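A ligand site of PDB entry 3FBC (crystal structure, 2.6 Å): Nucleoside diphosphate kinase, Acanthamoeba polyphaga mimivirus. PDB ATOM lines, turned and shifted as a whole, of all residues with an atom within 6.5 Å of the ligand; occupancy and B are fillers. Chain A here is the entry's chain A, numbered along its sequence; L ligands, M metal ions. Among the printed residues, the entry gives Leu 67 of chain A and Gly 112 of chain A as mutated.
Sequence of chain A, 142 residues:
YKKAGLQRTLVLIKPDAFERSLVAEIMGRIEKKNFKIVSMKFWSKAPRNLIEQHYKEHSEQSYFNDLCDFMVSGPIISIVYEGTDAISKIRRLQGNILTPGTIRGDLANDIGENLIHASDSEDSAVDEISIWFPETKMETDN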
ATOM      1  N   LYS A  14     -29.858 -13.242 -22.323  1.00  0.00           N
ATOM      2  CA  LYS A  14     -29.099 -12.301 -21.512  1.00  0.00           C
ATOM      3  C   LYS A  14     -28.229 -11.354 -22.354  1.00  0.00           C
ATOM      4  O   LYS A  14     -28.081 -11.555 -23.559  1.00  0.00           O
ATOM      5  CB  LYS A  14     -28.240 -13.079 -20.505  1.00  0.00           C
ATOM      6  CG  LYS A  14     -29.058 -14.012 -19.623  1.00  0.00           C
ATOM      7  CD  LYS A  14     -28.216 -14.602 -18.520  1.00  0.00           C
ATOM      8  CE  LYS A  14     -29.099 -15.364 -17.541  1.00  0.00           C
ATOM      9  NZ  LYS A  14     -28.293 -16.235 -16.648  1.00  0.00           N
ATOM     10  N   TYR A  55     -34.647 -12.673  -9.748  1.00  0.00           N
ATOM     11  CA  TYR A  55     -33.610 -13.347  -8.984  1.00  0.00           C
ATOM     12  C   TYR A  55     -33.762 -13.086  -7.478  1.00  0.00           C
ATOM     13  O   TYR A  55     -32.767 -12.963  -6.753  1.00  0.00           O
ATOM     14  CB  TYR A  55     -32.231 -12.901  -9.471  1.00  0.00           C
ATOM     15  CG  TYR A  55     -31.822 -13.489 -10.812  1.00  0.00           C
ATOM     16  CD1 TYR A  55     -31.507 -12.671 -11.892  1.00  0.00           C
ATOM     17  CD2 TYR A  55     -31.753 -14.864 -10.984  1.00  0.00           C
ATOM     18  CE1 TYR A  55     -31.137 -13.219 -13.111  1.00  0.00           C
ATOM     19  CE2 TYR A  55     -31.383 -15.411 -12.203  1.00  0.00           C
ATOM     20  CZ  TYR A  55     -31.077 -14.592 -13.260  1.00  0.00           C
ATOM     21  OH  TYR A  55     -30.718 -15.159 -14.460  1.00  0.00           O
ATOM     22  N   HIS A  58     -32.135 -15.383  -5.029  1.00  0.00           N
ATOM     23  CA  HIS A  58     -30.689 -15.246  -4.911  1.00  0.00           C
ATOM     24  C   HIS A  58     -30.267 -13.992  -4.151  1.00  0.00           C
ATOM     25  O   HIS A  58     -29.090 -13.676  -4.103  1.00  0.00           O
ATOM     26  CB  HIS A  58     -30.032 -15.215  -6.297  1.00  0.00           C
ATOM     27  CG  HIS A  58     -30.365 -16.390  -7.161  1.00  0.00           C
ATOM     28  ND1 HIS A  58     -29.448 -17.389  -7.441  1.00  0.00           N
ATOM     29  CD2 HIS A  58     -31.498 -16.727  -7.816  1.00  0.00           C
ATOM     30  CE1 HIS A  58     -30.006 -18.288  -8.220  1.00  0.00           C
ATOM     31  NE2 HIS A  58     -31.252 -17.917  -8.472  1.00  0.00           N
ATOM     32  N   GLN A  61     -27.133 -13.832  -1.757  1.00  0.00           N
ATOM     33  CA  GLN A  61     -25.902 -14.440  -2.248  1.00  0.00           C
ATOM     34  C   GLN A  61     -24.793 -13.429  -2.455  1.00  0.00           C
ATOM     35  O   GLN A  61     -25.053 -12.230  -2.585  1.00  0.00           O
ATOM     36  CB  GLN A  61     -26.174 -15.170  -3.563  1.00  0.00           C
ATOM     37  CG  GLN A  61     -27.098 -16.355  -3.395  1.00  0.00           C
ATOM     38  CD  GLN A  61     -26.528 -17.366  -2.438  1.00  0.00           C
ATOM     39  OE1 GLN A  61     -25.406 -17.868  -2.625  1.00  0.00           O
ATOM     40  NE2 GLN A  61     -27.284 -17.680  -1.392  1.00  0.00           N
ATOM     41  N   SER A  62     -23.554 -13.908  -2.483  1.00  0.00           N
ATOM     42  CA  SER A  62     -22.399 -13.047  -2.725  1.00  0.00           C
ATOM     43  C   SER A  62     -22.525 -12.397  -4.105  1.00  0.00           C
ATOM     44  O   SER A  62     -22.248 -11.199  -4.274  1.00  0.00           O
ATOM     45  CB  SER A  62     -21.095 -13.845  -2.624  1.00  0.00           C
ATOM     46  OG  SER A  62     -21.172 -15.085  -3.333  1.00  0.00           O
ATOM     47  N   TYR A  63     -22.963 -13.204  -5.069  1.00  0.00           N
ATOM     48  CA  TYR A  63     -23.019 -12.807  -6.461  1.00  0.00           C
ATOM     49  C   TYR A  63     -24.261 -12.014  -6.832  1.00  0.00           C
ATOM     50  O   TYR A  63     -24.458 -11.714  -7.998  1.00  0.00           O
ATOM     51  CB  TYR A  63     -22.950 -14.059  -7.349  1.00  0.00           C
ATOM     52  CG  TYR A  63     -24.029 -15.075  -7.059  1.00  0.00           C
ATOM     53  CD1 TYR A  63     -25.351 -14.840  -7.421  1.00  0.00           C
ATOM     54  CD2 TYR A  63     -23.722 -16.283  -6.439  1.00  0.00           C
ATOM     55  CE1 TYR A  63     -26.339 -15.776  -7.159  1.00  0.00           C
ATOM     56  CE2 TYR A  63     -24.707 -17.211  -6.172  1.00  0.00           C
ATOM     57  CZ  TYR A  63     -26.004 -16.961  -6.535  1.00  0.00           C
ATOM     58  OH  TYR A  63     -26.980 -17.890  -6.274  1.00  0.00           O
ATOM     59  N   ASP A  66     -23.520  -8.284  -8.681  1.00  0.00           N
ATOM     60  CA  ASP A  66     -22.856  -8.440  -9.960  1.00  0.00           C
ATOM     61  C   ASP A  66     -23.803  -9.110 -10.956  1.00  0.00           C
ATOM     62  O   ASP A  66     -23.769  -8.817 -12.154  1.00  0.00           O
ATOM     63  CB  ASP A  66     -21.570  -9.245  -9.795  1.00  0.00           C
ATOM     64  CG  ASP A  66     -20.645  -8.631  -8.775  1.00  0.00           C
ATOM     65  OD1 ASP A  66     -20.582  -7.377  -8.725  1.00  0.00           O
ATOM     66  OD2 ASP A  66     -19.988  -9.395  -8.021  1.00  0.00           O
ATOM     67  N   LEU A  67     -24.653 -10.000 -10.451  1.00  0.00           N
ATOM     68  CA  LEU A  67     -25.669 -10.632 -11.262  1.00  0.00           C
ATOM     69  C   LEU A  67     -26.553  -9.544 -11.826  1.00  0.00           C
ATOM     70  O   LEU A  67     -26.655  -9.381 -13.044  1.00  0.00           O
ATOM     71  CB  LEU A  67     -26.532 -11.563 -10.410  1.00  0.00           C
ATOM     72  CG  LEU A  67     -27.146 -12.752 -11.137  1.00  0.00           C
ATOM     73  CD1 LEU A  67     -28.411 -13.168 -10.423  1.00  0.00           C
ATOM     74  CD2 LEU A  67     -27.443 -12.413 -12.566  1.00  0.00           C
ATOM     75  N   ARG A  91     -35.012 -26.473 -20.191  1.00  0.00           N
ATOM     76  CA  ARG A  91     -33.986 -26.514 -19.157  1.00  0.00           C
ATOM     77  C   ARG A  91     -32.771 -27.328 -19.575  1.00  0.00           C
ATOM     78  O   ARG A  91     -31.636 -26.961 -19.301  1.00  0.00           O
ATOM     79  CB  ARG A  91     -34.565 -27.079 -17.869  1.00  0.00           C
ATOM     80  CG  ARG A  91     -34.623 -26.080 -16.757  1.00  0.00           C
ATOM     81  CD  ARG A  91     -33.293 -26.047 -16.028  1.00  0.00           C
ATOM     82  NE  ARG A  91     -33.002 -24.718 -15.507  1.00  0.00           N
ATOM     83  CZ  ARG A  91     -32.153 -24.472 -14.516  1.00  0.00           C
ATOM     84  NH1 ARG A  91     -31.519 -25.482 -13.916  1.00  0.00           N
ATOM     85  NH2 ARG A  91     -31.949 -23.223 -14.106  1.00  0.00           N
ATOM     86  N   GLN A  94     -30.808 -25.545 -22.261  1.00  0.00           N
ATOM     87  CA  GLN A  94     -29.923 -24.550 -21.661  1.00  0.00           C
ATOM     88  C   GLN A  94     -28.650 -25.170 -21.086  1.00  0.00           C
ATOM     89  O   GLN A  94     -27.564 -24.617 -21.240  1.00  0.00           O
ATOM     90  CB  GLN A  94     -30.652 -23.763 -20.579  1.00  0.00           C
ATOM     91  CG  GLN A  94     -29.748 -23.283 -19.477  1.00  0.00           C
ATOM     92  CD  GLN A  94     -30.532 -22.698 -18.323  1.00  0.00           C
ATOM     93  OE1 GLN A  94     -31.097 -21.612 -18.440  1.00  0.00           O
ATOM     94  NE2 GLN A  94     -30.571 -23.406 -17.210  1.00  0.00           N
ATOM     95  N   GLY A  95     -28.801 -26.316 -20.419  1.00  0.00           N
ATOM     96  CA  GLY A  95     -27.669 -27.086 -19.926  1.00  0.00           C
ATOM     97  C   GLY A  95     -26.746 -26.294 -19.042  1.00  0.00           C
ATOM     98  O   GLY A  95     -27.172 -25.358 -18.360  1.00  0.00           O
ATOM     99  N   ARG A 104     -25.405 -23.612 -23.164  1.00  0.00           N
ATOM    100  CA  ARG A 104     -24.268 -23.196 -22.360  1.00  0.00           C
ATOM    101  C   ARG A 104     -23.070 -24.085 -22.672  1.00  0.00           C
ATOM    102  O   ARG A 104     -21.950 -23.609 -22.770  1.00  0.00           O
ATOM    103  CB  ARG A 104     -24.623 -23.210 -20.878  1.00  0.00           C
ATOM    104  CG  ARG A 104     -25.447 -22.008 -20.465  1.00  0.00           C
ATOM    105  CD  ARG A 104     -25.797 -22.030 -18.993  1.00  0.00           C
ATOM    106  NE  ARG A 104     -26.821 -21.045 -18.657  1.00  0.00           N
ATOM    107  CZ  ARG A 104     -27.594 -21.107 -17.574  1.00  0.00           C
ATOM    108  NH1 ARG A 104     -27.471 -22.122 -16.731  1.00  0.00           N
ATOM    109  NH2 ARG A 104     -28.510 -20.178 -17.344  1.00  0.00           N
ATOM    110  N   ASP A 110     -18.518 -19.126 -18.753  1.00  0.00           N
ATOM    111  CA  ASP A 110     -18.416 -18.369 -17.516  1.00  0.00           C
ATOM    112  C   ASP A 110     -19.605 -18.618 -16.603  1.00  0.00           C
ATOM    113  O   ASP A 110     -20.745 -18.699 -17.058  1.00  0.00           O
ATOM    114  CB  ASP A 110     -18.338 -16.869 -17.834  1.00  0.00           C
ATOM    115  CG  ASP A 110     -17.846 -16.044 -16.661  1.00  0.00           C
ATOM    116  OD1 ASP A 110     -18.611 -15.179 -16.163  1.00  0.00           O
ATOM    117  OD2 ASP A 110     -16.698 -16.278 -16.218  1.00  0.00           O
ATOM    118  N   ILE A 111     -19.339 -18.745 -15.302  1.00  0.00           N
ATOM    119  CA  ILE A 111     -20.386 -18.935 -14.302  1.00  0.00           C
ATOM    120  C   ILE A 111     -21.496 -17.918 -14.425  1.00  0.00           C
ATOM    121  O   ILE A 111     -22.651 -18.243 -14.240  1.00  0.00           O
ATOM    122  CB  ILE A 111     -19.844 -18.777 -12.865  1.00  0.00           C
ATOM    123  CG1 ILE A 111     -18.685 -17.754 -12.851  1.00  0.00           C
ATOM    124  CG2 ILE A 111     -19.438 -20.142 -12.288  1.00  0.00           C
ATOM    125  CD1 ILE A 111     -17.919 -17.664 -11.543  1.00  0.00           C
ATOM    126  N   GLY A 112     -21.127 -16.675 -14.747  1.00  0.00           N
ATOM    127  CA  GLY A 112     -22.065 -15.566 -14.757  1.00  0.00           C
ATOM    128  C   GLY A 112     -22.569 -15.138 -16.121  1.00  0.00           C
ATOM    129  O   GLY A 112     -23.776 -14.915 -16.309  1.00  0.00           O
ATOM    130  N   GLU A 113     -21.666 -15.021 -17.083  1.00  0.00           N
ATOM    131  CA  GLU A 113     -22.051 -14.606 -18.430  1.00  0.00           C
ATOM    132  C   GLU A 113     -22.462 -15.828 -19.228  1.00  0.00           C
ATOM    133  O   GLU A 113     -21.683 -16.386 -19.990  1.00  0.00           O
ATOM    134  CB  GLU A 113     -20.914 -13.872 -19.113  1.00  0.00           C
ATOM    135  CG  GLU A 113     -20.277 -12.828 -18.218  1.00  0.00           C
ATOM    136  CD  GLU A 113     -19.661 -11.678 -18.980  1.00  0.00           C
ATOM    137  OE1 GLU A 113     -19.008 -11.937 -20.016  1.00  0.00           O
ATOM    138  OE2 GLU A 113     -19.818 -10.520 -18.533  1.00  0.00           O
ATOM    139  N   ASN A 114     -23.713 -16.253 -19.059  1.00  0.00           N
ATOM    140  CA  ASN A 114     -24.083 -17.551 -19.591  1.00  0.00           C
ATOM    141  C   ASN A 114     -25.276 -17.574 -20.549  1.00  0.00           C
ATOM    142  O   ASN A 114     -25.945 -18.595 -20.691  1.00  0.00           O
ATOM    143  CB  ASN A 114     -24.219 -18.607 -18.486  1.00  0.00           C
ATOM    144  CG  ASN A 114     -25.262 -18.239 -17.463  1.00  0.00           C
ATOM    145  OD1 ASN A 114     -26.046 -17.301 -17.671  1.00  0.00           O
ATOM    146  ND2 ASN A 114     -25.303 -18.986 -16.369  1.00  0.00           N
ATOM    147  N   ILE A 116     -28.346 -17.395 -21.274  1.00  0.00           N
ATOM    148  CA  ILE A 116     -29.770 -17.687 -21.189  1.00  0.00           C
ATOM    149  C   ILE A 116     -30.275 -18.139 -19.811  1.00  0.00           C
ATOM    150  O   ILE A 116     -29.634 -18.936 -19.153  1.00  0.00           O
ATOM    151  CB  ILE A 116     -30.130 -18.776 -22.225  1.00  0.00           C
ATOM    152  CG1 ILE A 116     -31.621 -19.084 -22.204  1.00  0.00           C
ATOM    153  CG2 ILE A 116     -29.367 -20.058 -21.964  1.00  0.00           C
ATOM    154  CD1 ILE A 116     -31.964 -20.157 -23.161  1.00  0.00           C
ATOM    155  N   HIS A 117     -31.430 -17.615 -19.402  1.00  0.00           N
ATOM    156  CA  HIS A 117     -32.199 -18.194 -18.293  1.00  0.00           C
ATOM    157  C   HIS A 117     -33.405 -18.972 -18.788  1.00  0.00           C
ATOM    158  O   HIS A 117     -34.089 -18.557 -19.733  1.00  0.00           O
ATOM    159  CB  HIS A 117     -32.710 -17.114 -17.362  1.00  0.00           C
ATOM    160  CG  HIS A 117     -33.676 -17.626 -16.337  1.00  0.00           C
ATOM    161  ND1 HIS A 117     -33.290 -18.022 -15.079  1.00  0.00           N
ATOM    162  CD2 HIS A 117     -35.015 -17.809 -16.400  1.00  0.00           C
ATOM    163  CE1 HIS A 117     -34.344 -18.440 -14.410  1.00  0.00           C
ATOM    164  NE2 HIS A 117     -35.407 -18.315 -15.175  1.00  0.00           N
ATOM    165  N   ALA A 118     -33.667 -20.104 -18.143  1.00  0.00           N
ATOM    166  CA  ALA A 118     -34.904 -20.834 -18.377  1.00  0.00           C
ATOM    167  C   ALA A 118     -35.453 -21.285 -17.030  1.00  0.00           C
ATOM    168  O   ALA A 118     -34.699 -21.630 -16.125  1.00  0.00           O
ATOM    169  CB  ALA A 118     -34.674 -22.025 -19.295  1.00  0.00           C
ATOM    170  N   ASP A 120     -36.734 -23.208 -13.956  1.00  0.00           N
ATOM    171  CA  ASP A 120     -36.331 -24.535 -13.494  1.00  0.00           C
ATOM    172  C   ASP A 120     -37.476 -25.421 -12.965  1.00  0.00           C
ATOM    173  O   ASP A 120     -37.268 -26.613 -12.751  1.00  0.00           O
ATOM    174  CB  ASP A 120     -35.166 -24.468 -12.508  1.00  0.00           C
ATOM    175  CG  ASP A 120     -35.581 -24.001 -11.154  1.00  0.00           C
ATOM    176  OD1 ASP A 120     -36.800 -23.792 -10.940  1.00  0.00           O
ATOM    177  OD2 ASP A 120     -34.678 -23.846 -10.296  1.00  0.00           O
HETATM  178  P1  LIG L   1     -27.198 -20.462 -10.988  1.00  0.00           P
HETATM  179  O1  LIG L   1     -28.466 -20.765 -10.211  1.00  0.00           O
HETATM  180  O2  LIG L   1     -25.912 -21.193 -10.663  1.00  0.00           O
HETATM  181  O3  LIG L   1     -27.460 -20.645 -12.582  1.00  0.00           O
HETATM  182  P2  LIG L   1     -28.907 -20.706 -13.323  1.00  0.00           P
HETATM  183  O4  LIG L   1     -28.888 -19.526 -14.283  1.00  0.00           O
HETATM  184  O5  LIG L   1     -30.008 -20.575 -12.289  1.00  0.00           O
HETATM  185  O6  LIG L   1     -28.816 -22.074 -13.972  1.00  0.00           O
HETATM  186  O7  LIG L   1     -26.883 -18.878 -10.894  1.00  0.00           O
HETATM  187  C1  LIG L   1     -27.907 -17.895 -11.104  1.00  0.00           C
HETATM  188  C2  LIG L   1     -27.330 -16.782 -11.997  1.00  0.00           C
HETATM  189  O8  LIG L   1     -26.480 -15.932 -11.208  1.00  0.00           O
HETATM  190  C3  LIG L   1     -26.477 -17.382 -13.118  1.00  0.00           C
HETATM  191  O9  LIG L   1     -27.178 -17.427 -14.363  1.00  0.00           O
HETATM  192  C4  LIG L   1     -25.235 -16.504 -13.172  1.00  0.00           C
HETATM  193  C5  LIG L   1     -25.152 -15.908 -11.757  1.00  0.00           C
HETATM  194  N1  LIG L   1     -24.209 -16.639 -10.880  1.00  0.00           N
HETATM  195  C6  LIG L   1     -22.881 -16.159 -10.698  1.00  0.00           C
HETATM  196  O10 LIG L   1     -22.510 -15.115 -11.283  1.00  0.00           O
HETATM  197  N2  LIG L   1     -22.010 -16.809  -9.896  1.00  0.00           N
HETATM  198  C7  LIG L   1     -22.367 -17.924  -9.250  1.00  0.00           C
HETATM  199  O11 LIG L   1     -21.545 -18.525  -8.507  1.00  0.00           O
HETATM  200  C8  LIG L   1     -23.746 -18.454  -9.417  1.00  0.00           C
HETATM  201  C9  LIG L   1     -24.196 -19.709  -8.708  1.00  0.00           C
HETATM  202  C10 LIG L   1     -24.619 -17.750 -10.242  1.00  0.00           C
HETATM  203 MG    MG M   1     -31.425 -22.553 -11.132  1.00  0.00          MG
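Merely in contact with the ligand: Leu 67, Ile 111, Tyr 63, Gly 112, His 58 and Gln 94. Hydrophobic or aromatic side chains within 4 Å of the ligand: His 58, Tyr 63 and Leu 67. Of the 21 residues printed, 10 come within 4 Å of the ligand. The nearest printed residue that does not touch the ligand is Tyr 55 (4.2 Å).
NH2 of Arg 91 lies within salt-bridge range of O6 of the ligand (3.3 Å). An oxygen (O9) of the ligand is in hydrogen-bond range of the side-chain amino group (NZ) of Lys 14. NH1 of Arg 104 is in salt-bridge range of O6 of the ligand. The side-chain amide nitrogen of Asn 114 is in hydrogen-bond range of an oxygen (O9) of the ligand, 3.2 Å away.
The side-chain amide oxygen (OE1) of Gln 94 sits close to the backbone carbonyl oxygen (O) of Ile 116 (3.1 Å). O of Gln 94 lies within hydrogen-bond range of N of Arg 104, 3.1 Å away. The side-chain amino group of Lys 14 sits at hydrogen-bond distance from the side-chain amide oxygen of Asn 114. The guanidinium group (NE) of Arg 91 sits close to the side-chain amide nitrogen (NE2) of Gln 94 (3.2 Å). NZ of Lys 14 lies within hydrogen-bond range of OH of Tyr 55 (3.4 Å). ND1 of His 58 is in hydrogen-bond range of OH of Tyr 63, 2.8 Å away. NE of Arg 104 lies within hydrogen-bond range of O of Asn 114 (3.3 Å). The side-chain carboxylate (OD1) of Asp 110 lies close to the backbone NH (N) of Gly 112, 3.3 Å away.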
